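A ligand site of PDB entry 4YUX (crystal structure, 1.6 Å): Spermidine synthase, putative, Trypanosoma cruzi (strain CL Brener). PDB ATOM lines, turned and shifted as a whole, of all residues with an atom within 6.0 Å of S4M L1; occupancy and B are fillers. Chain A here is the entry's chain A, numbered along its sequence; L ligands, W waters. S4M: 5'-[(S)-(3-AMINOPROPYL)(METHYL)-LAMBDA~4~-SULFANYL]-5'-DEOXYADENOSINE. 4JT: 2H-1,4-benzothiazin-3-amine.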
ATOM      1  N   GLN A  48      10.087  20.272  -2.833  1.00  0.00           N
ATOM      2  CA  GLN A  48      11.103  20.818  -3.762  1.00  0.00           C
ATOM      3  C   GLN A  48      12.262  21.274  -2.983  1.00  0.00           C
ATOM      4  O   GLN A  48      12.149  21.460  -1.784  1.00  0.00           O
ATOM      5  CB  GLN A  48      10.536  21.983  -4.559  1.00  0.00           C
ATOM      6  CG  GLN A  48       9.435  21.562  -5.543  1.00  0.00           C
ATOM      7  CD  GLN A  48       8.695  22.754  -6.145  1.00  0.00           C
ATOM      8  OE1 GLN A  48       8.777  23.034  -7.324  1.00  0.00           O
ATOM      9  NE2 GLN A  48       7.969  23.537  -5.289  1.00  0.00           N
ATOM     10  N   MET A  65      15.631  33.515  -6.162  1.00  0.00           N
ATOM     11  CA  MET A  65      15.011  32.291  -5.642  1.00  0.00           C
ATOM     12  C   MET A  65      15.178  31.167  -6.657  1.00  0.00           C
ATOM     13  O   MET A  65      15.026  31.410  -7.851  1.00  0.00           O
ATOM     14  CB  MET A  65      13.474  32.514  -5.488  1.00  0.00           C
ATOM     15  CG  MET A  65      12.817  31.198  -5.073  1.00  0.00           C
ATOM     16  SD  MET A  65      10.956  31.341  -5.196  1.00  0.00           S
ATOM     17  CE  MET A  65      10.781  32.579  -3.939  1.00  0.00           C
ATOM     18  N   LEU A  67      14.116  26.864  -7.350  1.00  0.00           N
ATOM     19  CA  LEU A  67      13.414  25.634  -6.933  1.00  0.00           C
ATOM     20  C   LEU A  67      13.979  24.477  -7.728  1.00  0.00           C
ATOM     21  O   LEU A  67      14.068  24.527  -8.973  1.00  0.00           O
ATOM     22  CB  LEU A  67      11.903  25.701  -7.279  1.00  0.00           C
ATOM     23  CG  LEU A  67      11.139  26.575  -6.237  1.00  0.00           C
ATOM     24  CD1 LEU A  67       9.683  26.755  -6.803  1.00  0.00           C
ATOM     25  CD2 LEU A  67      11.024  25.780  -4.948  1.00  0.00           C
ATOM     26  N   GLN A  72      13.929  30.935 -10.366  1.00  0.00           N
ATOM     27  CA  GLN A  72      12.460  31.201 -10.503  1.00  0.00           C
ATOM     28  C   GLN A  72      12.157  32.688 -10.650  1.00  0.00           C
ATOM     29  O   GLN A  72      11.263  33.074 -11.412  1.00  0.00           O
ATOM     30  CB  GLN A  72      11.724  30.752  -9.269  1.00  0.00           C
ATOM     31  CG  GLN A  72      11.810  29.218  -9.012  1.00  0.00           C
ATOM     32  CD  GLN A  72      11.172  28.402 -10.118  1.00  0.00           C
ATOM     33  OE1 GLN A  72       9.935  28.476 -10.330  1.00  0.00           O
ATOM     34  NE2 GLN A  72      11.963  27.594 -10.777  1.00  0.00           N
ATOM     35  N   VAL A  73      12.836  33.483  -9.793  1.00  0.00           N
ATOM     36  CA  VAL A  73      12.657  34.942  -9.825  1.00  0.00           C
ATOM     37  C   VAL A  73      13.993  35.583  -9.370  1.00  0.00           C
ATOM     38  O   VAL A  73      14.745  35.008  -8.649  1.00  0.00           O
ATOM     39  CB  VAL A  73      11.544  35.532  -8.951  1.00  0.00           C
ATOM     40  CG1 VAL A  73      10.096  35.150  -9.423  1.00  0.00           C
ATOM     41  CG2 VAL A  73      11.745  35.099  -7.511  1.00  0.00           C
ATOM     42  N   TYR A  81       8.002  38.298 -16.820  1.00  0.00           N
ATOM     43  CA  TYR A  81       7.111  37.203 -17.003  1.00  0.00           C
ATOM     44  C   TYR A  81       5.789  37.442 -16.250  1.00  0.00           C
ATOM     45  O   TYR A  81       4.719  37.092 -16.697  1.00  0.00           O
ATOM     46  CB  TYR A  81       7.890  35.959 -16.571  1.00  0.00           C
ATOM     47  CG  TYR A  81       7.058  34.716 -16.332  1.00  0.00           C
ATOM     48  CD1 TYR A  81       6.453  34.460 -15.109  1.00  0.00           C
ATOM     49  CD2 TYR A  81       6.928  33.772 -17.348  1.00  0.00           C
ATOM     50  CE1 TYR A  81       5.794  33.272 -14.926  1.00  0.00           C
ATOM     51  CE2 TYR A  81       6.316  32.552 -17.191  1.00  0.00           C
ATOM     52  CZ  TYR A  81       5.751  32.304 -15.971  1.00  0.00           C
ATOM     53  OH  TYR A  81       5.074  31.109 -15.723  1.00  0.00           O
ATOM     54  N   HIS A  82       5.900  38.107 -15.093  1.00  0.00           N
ATOM     55  CA  HIS A  82       4.659  38.389 -14.358  1.00  0.00           C
ATOM     56  C   HIS A  82       3.744  39.352 -15.101  1.00  0.00           C
ATOM     57  O   HIS A  82       2.549  39.074 -15.198  1.00  0.00           O
ATOM     58  CB  HIS A  82       5.054  38.917 -12.978  1.00  0.00           C
ATOM     59  CG  HIS A  82       5.756  37.890 -12.176  1.00  0.00           C
ATOM     60  ND1 HIS A  82       6.682  38.182 -11.180  1.00  0.00           N
ATOM     61  CD2 HIS A  82       5.650  36.538 -12.204  1.00  0.00           C
ATOM     62  CE1 HIS A  82       7.098  37.030 -10.634  1.00  0.00           C
ATOM     63  NE2 HIS A  82       6.460  36.046 -11.236  1.00  0.00           N
ATOM     64  N   ILE A 102      -2.740  28.636 -11.248  1.00  0.00           N
ATOM     65  CA  ILE A 102      -2.130  27.362 -10.797  1.00  0.00           C
ATOM     66  C   ILE A 102      -0.610  27.558 -10.713  1.00  0.00           C
ATOM     67  O   ILE A 102      -0.008  28.115 -11.591  1.00  0.00           O
ATOM     68  CB  ILE A 102      -2.474  26.222 -11.798  1.00  0.00           C
ATOM     69  CG1 ILE A 102      -4.011  26.007 -11.844  1.00  0.00           C
ATOM     70  CG2 ILE A 102      -1.713  24.918 -11.398  1.00  0.00           C
ATOM     71  CD1 ILE A 102      -4.622  25.597 -10.492  1.00  0.00           C
ATOM     72  N   GLY A 103      -0.043  27.218  -9.558  1.00  0.00           N
ATOM     73  CA  GLY A 103       1.309  27.559  -9.204  1.00  0.00           C
ATOM     74  C   GLY A 103       1.362  29.030  -8.729  1.00  0.00           C
ATOM     75  O   GLY A 103       0.522  29.457  -7.932  1.00  0.00           O
ATOM     76  N   GLY A 104       2.375  29.776  -9.178  1.00  0.00           N
ATOM     77  CA  GLY A 104       2.377  31.240  -8.806  1.00  0.00           C
ATOM     78  C   GLY A 104       2.569  31.616  -7.386  1.00  0.00           C
ATOM     79  O   GLY A 104       2.155  32.657  -6.973  1.00  0.00           O
ATOM     80  N   GLY A 105       3.110  30.683  -6.568  1.00  0.00           N
ATOM     81  CA  GLY A 105       3.152  30.882  -5.100  1.00  0.00           C
ATOM     82  C   GLY A 105       4.022  32.084  -4.702  1.00  0.00           C
ATOM     83  O   GLY A 105       3.876  32.535  -3.583  1.00  0.00           O
ATOM     84  N   ASP A 106       4.948  32.576  -5.579  1.00  0.00           N
ATOM     85  CA  ASP A 106       5.687  33.812  -5.247  1.00  0.00           C
ATOM     86  C   ASP A 106       4.752  35.062  -5.249  1.00  0.00           C
ATOM     87  O   ASP A 106       5.151  36.071  -4.638  1.00  0.00           O
ATOM     88  CB  ASP A 106       6.822  34.067  -6.262  1.00  0.00           C
ATOM     89  CG  ASP A 106       6.366  33.901  -7.678  1.00  0.00           C
ATOM     90  OD1 ASP A 106       5.676  34.747  -8.186  1.00  0.00           O
ATOM     91  OD2 ASP A 106       6.661  32.843  -8.299  1.00  0.00           O
ATOM     92  N   GLY A 108       3.768  36.846  -7.960  1.00  0.00           N
ATOM     93  CA  GLY A 108       3.970  37.896  -9.025  1.00  0.00           C
ATOM     94  C   GLY A 108       2.856  37.977 -10.012  1.00  0.00           C
ATOM     95  O   GLY A 108       2.412  39.115 -10.352  1.00  0.00           O
ATOM     96  N   VAL A 109       2.426  36.846 -10.573  1.00  0.00           N
ATOM     97  CA  VAL A 109       1.294  36.898 -11.495  1.00  0.00           C
ATOM     98  C   VAL A 109       0.031  37.466 -10.818  1.00  0.00           C
ATOM     99  O   VAL A 109      -0.656  38.278 -11.391  1.00  0.00           O
ATOM    100  CB  VAL A 109       1.025  35.481 -12.116  1.00  0.00           C
ATOM    101  CG1 VAL A 109      -0.294  35.512 -12.939  1.00  0.00           C
ATOM    102  CG2 VAL A 109       2.232  35.109 -12.993  1.00  0.00           C
ATOM    103  N   VAL A 125      -3.466  28.416  -6.411  1.00  0.00           N
ATOM    104  CA  VAL A 125      -3.338  27.077  -5.796  1.00  0.00           C
ATOM    105  C   VAL A 125      -1.941  26.624  -6.181  1.00  0.00           C
ATOM    106  O   VAL A 125      -1.658  26.343  -7.373  1.00  0.00           O
ATOM    107  CB  VAL A 125      -4.313  26.070  -6.426  1.00  0.00           C
ATOM    108  CG1 VAL A 125      -4.152  24.743  -5.615  1.00  0.00           C
ATOM    109  CG2 VAL A 125      -5.749  26.614  -6.143  1.00  0.00           C
ATOM    110  N   ASP A 126      -1.041  26.644  -5.200  1.00  0.00           N
ATOM    111  CA  ASP A 126       0.304  26.213  -5.443  1.00  0.00           C
ATOM    112  C   ASP A 126       0.619  24.995  -4.486  1.00  0.00           C
ATOM    113  O   ASP A 126       0.211  25.056  -3.277  1.00  0.00           O
ATOM    114  CB  ASP A 126       1.297  27.390  -5.080  1.00  0.00           C
ATOM    115  CG  ASP A 126       2.711  27.095  -5.502  1.00  0.00           C
ATOM    116  OD1 ASP A 126       3.297  26.045  -5.123  1.00  0.00           O
ATOM    117  OD2 ASP A 126       3.330  27.879  -6.360  1.00  0.00           O
ATOM    118  N   ILE A 127       1.326  23.980  -5.007  1.00  0.00           N
ATOM    119  CA  ILE A 127       1.496  22.738  -4.186  1.00  0.00           C
ATOM    120  C   ILE A 127       2.382  23.031  -3.009  1.00  0.00           C
ATOM    121  O   ILE A 127       2.289  22.243  -1.960  1.00  0.00           O
ATOM    122  CB  ILE A 127       2.014  21.593  -5.106  1.00  0.00           C
ATOM    123  CG1 ILE A 127       1.909  20.242  -4.367  1.00  0.00           C
ATOM    124  CG2 ILE A 127       3.499  21.832  -5.493  1.00  0.00           C
ATOM    125  CD1 ILE A 127       2.281  19.166  -5.395  1.00  0.00           C
ATOM    126  N   ASP A 128       3.257  23.996  -3.089  1.00  0.00           N
ATOM    127  CA  ASP A 128       4.313  24.195  -2.110  1.00  0.00           C
ATOM    128  C   ASP A 128       4.149  25.389  -1.242  1.00  0.00           C
ATOM    129  O   ASP A 128       4.488  26.473  -1.644  1.00  0.00           O
ATOM    130  CB  ASP A 128       5.657  24.191  -2.839  1.00  0.00           C
ATOM    131  CG  ASP A 128       6.835  23.926  -1.891  1.00  0.00           C
ATOM    132  OD1 ASP A 128       6.712  24.223  -0.672  1.00  0.00           O
ATOM    133  OD2 ASP A 128       7.871  23.387  -2.383  1.00  0.00           O
ATOM    134  N   VAL A 131       6.909  28.055  -0.648  1.00  0.00           N
ATOM    135  CA  VAL A 131       7.177  29.129  -1.611  1.00  0.00           C
ATOM    136  C   VAL A 131       6.465  30.414  -1.212  1.00  0.00           C
ATOM    137  O   VAL A 131       7.016  31.512  -1.237  1.00  0.00           O
ATOM    138  CB  VAL A 131       6.716  28.721  -3.022  1.00  0.00           C
ATOM    139  CG1 VAL A 131       6.968  29.899  -3.998  1.00  0.00           C
ATOM    140  CG2 VAL A 131       7.541  27.533  -3.546  1.00  0.00           C
ATOM    141  N   GLY A 156      -1.975  23.246  -2.371  1.00  0.00           N
ATOM    142  CA  GLY A 156      -2.464  21.950  -2.922  1.00  0.00           C
ATOM    143  C   GLY A 156      -1.973  21.762  -4.329  1.00  0.00           C
ATOM    144  O   GLY A 156      -1.575  22.713  -5.062  1.00  0.00           O
ATOM    145  N   ASP A 157      -2.086  20.499  -4.801  1.00  0.00           N
ATOM    146  CA  ASP A 157      -1.781  20.253  -6.192  1.00  0.00           C
ATOM    147  C   ASP A 157      -2.795  20.781  -7.214  1.00  0.00           C
ATOM    148  O   ASP A 157      -4.005  20.680  -6.991  1.00  0.00           O
ATOM    149  CB  ASP A 157      -1.717  18.688  -6.380  1.00  0.00           C
ATOM    150  CG  ASP A 157      -1.680  18.301  -7.805  1.00  0.00           C
ATOM    151  OD1 ASP A 157      -0.787  18.662  -8.551  1.00  0.00           O
ATOM    152  OD2 ASP A 157      -2.614  17.619  -8.254  1.00  0.00           O
ATOM    153  N   GLY A 158      -2.322  21.467  -8.251  1.00  0.00           N
ATOM    154  CA  GLY A 158      -3.219  22.021  -9.259  1.00  0.00           C
ATOM    155  C   GLY A 158      -4.102  21.025  -9.981  1.00  0.00           C
ATOM    156  O   GLY A 158      -5.239  21.377 -10.354  1.00  0.00           O
ATOM    157  N   LEU A 159      -3.580  19.820 -10.241  1.00  0.00           N
ATOM    158  CA  LEU A 159      -4.403  18.821 -10.961  1.00  0.00           C
ATOM    159  C   LEU A 159      -5.605  18.348 -10.109  1.00  0.00           C
ATOM    160  O   LEU A 159      -6.705  18.342 -10.605  1.00  0.00           O
ATOM    161  CB  LEU A 159      -3.582  17.598 -11.339  1.00  0.00           C
ATOM    162  CG  LEU A 159      -4.390  16.574 -12.183  1.00  0.00           C
ATOM    163  CD1 LEU A 159      -5.149  17.100 -13.432  1.00  0.00           C
ATOM    164  CD2 LEU A 159      -3.322  15.493 -12.505  1.00  0.00           C
ATOM    165  N   ASP A 176       1.130  28.984 -13.962  1.00  0.00           N
ATOM    166  CA  ASP A 176       2.525  29.540 -13.727  1.00  0.00           C
ATOM    167  C   ASP A 176       3.278  28.518 -12.959  1.00  0.00           C
ATOM    168  O   ASP A 176       3.371  28.546 -11.693  1.00  0.00           O
ATOM    169  CB  ASP A 176       2.452  30.906 -12.948  1.00  0.00           C
ATOM    170  CG  ASP A 176       3.823  31.313 -12.492  1.00  0.00           C
ATOM    171  OD1 ASP A 176       4.812  30.835 -13.000  1.00  0.00           O
ATOM    172  OD2 ASP A 176       3.968  32.174 -11.628  1.00  0.00           O
ATOM    173  N   THR A 177       3.871  27.562 -13.682  1.00  0.00           N
ATOM    174  CA  THR A 177       4.498  26.410 -13.007  1.00  0.00           C
ATOM    175  C   THR A 177       6.028  26.474 -13.149  1.00  0.00           C
ATOM    176  O   THR A 177       6.577  27.129 -14.075  1.00  0.00           O
ATOM    177  CB  THR A 177       4.025  25.094 -13.611  1.00  0.00           C
ATOM    178  OG1 THR A 177       4.391  25.057 -15.009  1.00  0.00           O
ATOM    179  CG2 THR A 177       2.508  24.979 -13.527  1.00  0.00           C
ATOM    180  N   THR A 178       6.656  25.673 -12.315  1.00  0.00           N
ATOM    181  CA  THR A 178       8.054  25.210 -12.591  1.00  0.00           C
ATOM    182  C   THR A 178       8.106  24.345 -13.874  1.00  0.00           C
ATOM    183  O   THR A 178       7.105  24.021 -14.543  1.00  0.00           O
ATOM    184  CB  THR A 178       8.543  24.360 -11.409  1.00  0.00           C
ATOM    185  OG1 THR A 178       7.480  23.453 -11.024  1.00  0.00           O
ATOM    186  CG2 THR A 178       8.872  25.196 -10.154  1.00  0.00           C
ATOM    187  N   GLY A 182       9.925  17.529 -11.723  1.00  0.00           N
ATOM    188  CA  GLY A 182       9.408  17.988 -10.416  1.00  0.00           C
ATOM    189  C   GLY A 182       7.917  17.858 -10.322  1.00  0.00           C
ATOM    190  O   GLY A 182       7.329  17.140 -11.091  1.00  0.00           O
ATOM    191  N   PRO A 183       7.337  18.494  -9.305  1.00  0.00           N
ATOM    192  CA  PRO A 183       5.913  18.307  -9.025  1.00  0.00           C
ATOM    193  C   PRO A 183       5.042  18.879 -10.131  1.00  0.00           C
ATOM    194  O   PRO A 183       3.822  18.618 -10.100  1.00  0.00           O
ATOM    195  CB  PRO A 183       5.721  19.091  -7.710  1.00  0.00           C
ATOM    196  CG  PRO A 183       6.894  20.061  -7.649  1.00  0.00           C
ATOM    197  CD  PRO A 183       8.013  19.312  -8.273  1.00  0.00           C
ATOM    198  N   ALA A 184       5.594  19.658 -11.107  1.00  0.00           N
ATOM    199  CA  ALA A 184       4.704  20.166 -12.178  1.00  0.00           C
ATOM    200  C   ALA A 184       4.519  19.200 -13.342  1.00  0.00           C
ATOM    201  O   ALA A 184       3.762  19.495 -14.278  1.00  0.00           O
ATOM    202  CB  ALA A 184       5.305  21.449 -12.797  1.00  0.00           C
ATOM    203  N   SER A 185       5.109  18.004 -13.209  1.00  0.00           N
ATOM    204  CA  SER A 185       5.139  17.072 -14.390  1.00  0.00           C
ATOM    205  C   SER A 185       3.772  16.949 -15.070  1.00  0.00           C
ATOM    206  O   SER A 185       3.625  17.119 -16.314  1.00  0.00           O
ATOM    207  CB  SER A 185       5.591  15.679 -13.883  1.00  0.00           C
ATOM    208  OG  SER A 185       5.669  14.886 -15.031  1.00  0.00           O
ATOM    209  N   LEU A 187       1.207  18.769 -14.998  1.00  0.00           N
ATOM    210  CA  LEU A 187       0.590  20.019 -15.498  1.00  0.00           C
ATOM    211  C   LEU A 187       0.997  20.402 -16.891  1.00  0.00           C
ATOM    212  O   LEU A 187       0.557  21.430 -17.448  1.00  0.00           O
ATOM    213  CB  LEU A 187       0.939  21.190 -14.492  1.00  0.00           C
ATOM    214  CG  LEU A 187       0.486  20.856 -13.059  1.00  0.00           C
ATOM    215  CD1 LEU A 187       0.696  22.100 -12.181  1.00  0.00           C
ATOM    216  CD2 LEU A 187      -0.978  20.474 -13.053  1.00  0.00           C
HETATM  217  CA  S4M L   1       7.715  32.748 -11.685  1.00  0.00           C
HETATM  218  N   S4M L   1       6.513  33.228 -10.910  1.00  0.00           N
HETATM  219  CB  S4M L   1       8.336  31.443 -11.168  1.00  0.00           C
HETATM  220  CG  S4M L   1       7.405  30.205 -11.242  1.00  0.00           C
HETATM  221  SD  S4M L   1       6.425  29.891  -9.781  1.00  0.00           S
HETATM  222  CE  S4M L   1       7.665  29.893  -8.470  1.00  0.00           C
HETATM  223  C5' S4M L   1       6.222  28.079 -10.059  1.00  0.00           C
HETATM  224  C4' S4M L   1       5.314  27.439  -9.004  1.00  0.00           C
HETATM  225  O4' S4M L   1       4.804  26.233  -9.559  1.00  0.00           O
HETATM  226  C1' S4M L   1       4.480  25.414  -8.370  1.00  0.00           C
HETATM  227  C2' S4M L   1       5.791  25.503  -7.607  1.00  0.00           C
HETATM  228  O2' S4M L   1       5.613  25.081  -6.206  1.00  0.00           O
HETATM  229  C3' S4M L   1       6.187  26.975  -7.826  1.00  0.00           C
HETATM  230  O3' S4M L   1       5.948  27.770  -6.637  1.00  0.00           O
HETATM  231  N9  S4M L   1       4.018  24.071  -8.718  1.00  0.00           N
HETATM  232  C8  S4M L   1       4.762  22.994  -9.179  1.00  0.00           C
HETATM  233  N7  S4M L   1       4.039  21.926  -9.369  1.00  0.00           N
HETATM  234  C5  S4M L   1       2.762  22.264  -9.024  1.00  0.00           C
HETATM  235  C6  S4M L   1       1.565  21.563  -8.898  1.00  0.00           C
HETATM  236  N6  S4M L   1       1.495  20.193  -9.236  1.00  0.00           N
HETATM  237  C4  S4M L   1       2.719  23.599  -8.628  1.00  0.00           C
HETATM  238  N3  S4M L   1       1.661  24.257  -8.182  1.00  0.00           N
HETATM  239  C2  S4M L   1       0.512  23.533  -8.162  1.00  0.00           C
HETATM  240  N1  S4M L   1       0.464  22.225  -8.505  1.00  0.00           N
HETATM  241  C10 4JT L   2      10.060  28.931 -13.876  1.00  0.00           C
HETATM  242  C11 4JT L   2       8.919  29.431 -14.442  1.00  0.00           C
HETATM  243  C8  4JT L   2      11.207  29.710 -13.829  1.00  0.00           C
HETATM  244  C9  4JT L   2       8.925  30.709 -15.015  1.00  0.00           C
HETATM  245  C4  4JT L   2      11.206  31.005 -14.380  1.00  0.00           C
HETATM  246  C5  4JT L   2      10.084  31.467 -14.984  1.00  0.00           C
HETATM  247  C3  4JT L   2      12.394  33.052 -14.257  1.00  0.00           C
HETATM  248  C6  4JT L   2      11.180  33.854 -14.352  1.00  0.00           C
HETATM  249  N1  4JT L   2      12.387  31.759 -14.274  1.00  0.00           N
HETATM  250  N7  4JT L   2      13.564  33.742 -14.039  1.00  0.00           N
HETATM  251  S2  4JT L   2      10.165  33.112 -15.686  1.00  0.00           S
HETATM  252  O   HOH W   1       3.639  34.299  -9.896  1.00  0.00           O
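O of Gln 72 lies close to N1 of 4JT L2.
N7 of S4M L1 lies within hydrogen-bond range of N of Ala 184, 3.3 Å away.
A ring nitrogen (NE2) of His 82 sits at hydrogen-bond distance from a nitrogen (N) of S4M L1, at 2.8 Å.
N6 of S4M L1 is in hydrogen-bond range of O of Pro 183 (2.9 Å).
N of Ile 127 is in hydrogen-bond range of N3 of S4M L1, at 3.2 Å.
The backbone NH (N) of Thr 178 sits close to an oxygen (O4') of S4M L1 (3.4 Å).
N of S4M L1 lies within salt-bridge range of OD2 of Asp 106 (2.6 Å).
The side-chain carboxylate of Asp 126 lies within hydrogen-bond range of an oxygen (O3') of S4M L1 (2.6 Å).
The side-chain carboxylate (OD2) of Asp 176 lies within salt-bridge range of a nitrogen (N) of S4M L1 (2.8 Å).
The side-chain carboxylate (OD1) of Asp 157 is in hydrogen-bond range of a nitrogen (N6) of S4M L1, at 2.8 Å.
The backbone NH (N) of Gly 158 lies within hydrogen-bond range of a nitrogen (N1) of S4M L1 (2.9 Å).
The side-chain amide nitrogen (NE2) of Gln 48 lies within hydrogen-bond range of an oxygen (O2') of S4M L1.
O of Asp 176 sits at hydrogen-bond distance from N of Gly 104 (3.0 Å).
N of Asp 176 lies within hydrogen-bond range of O of Ile 102, at 2.8 Å.
The side-chain carboxylate of Asp 126 lies within hydrogen-bond range of the backbone NH of Asp 128 (2.9 Å).
N of Gly 156 sits at hydrogen-bond distance from O of Asp 126.
NE2 of Gln 48 is in hydrogen-bond range of OD2 of Asp 128 (2.9 Å).
The backbone carbonyl oxygen of Val 125 is in hydrogen-bond range of the backbone NH of Gly 103 (2.9 Å).
N of Ile 127 lies within hydrogen-bond range of O of Gly 156 (3.2 Å).
The backbone NH (N) of Leu 159 sits at hydrogen-bond distance from the side-chain carboxylate (OD2) of Asp 157.
Leu 67 touches S4M L1.
Gln 72 touches S4M L1 (OE1 to CG, 3.2 Å).
Tyr 81 touches S4M L1.
Gly 103 touches S4M L1 (CA to N3, 3.5 Å).
Gly 104 touches S4M L1.
Val 125 touches S4M L1.
Asp 128 touches S4M L1 (CB to O2', 3.5 Å).
Val 131 touches S4M L1 (CG2 to O3', 3.5 Å).
Gly 156 touches S4M L1.
Thr 177 touches S4M L1.
Leu 187 touches S4M L1 (CD1 to C6, 3.4 Å).
Hydrophobic or aromatic side chains that line S4M L1: Leu 67, Tyr 81, His 82, Ile 127, Val 131, Pro 183, Ala 184 and Leu 187.
Of the 31 residues printed, 22 come within 4 Å of S4M L1.
The nearest printed residue that does not touch S4M L1 is Gly 105 (4.1 Å).
Water W1 lies within hydrogen-bond range of the side-chain carboxylate of Asp 106 (2.7 Å), the side-chain carboxylate of Asp 176 (2.8 Å), the backbone NH of Val 109 (2.9 Å), the backbone NH of Gly 108 (3.2 Å) and a nitrogen (N) of S4M L1 (3.2 Å).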
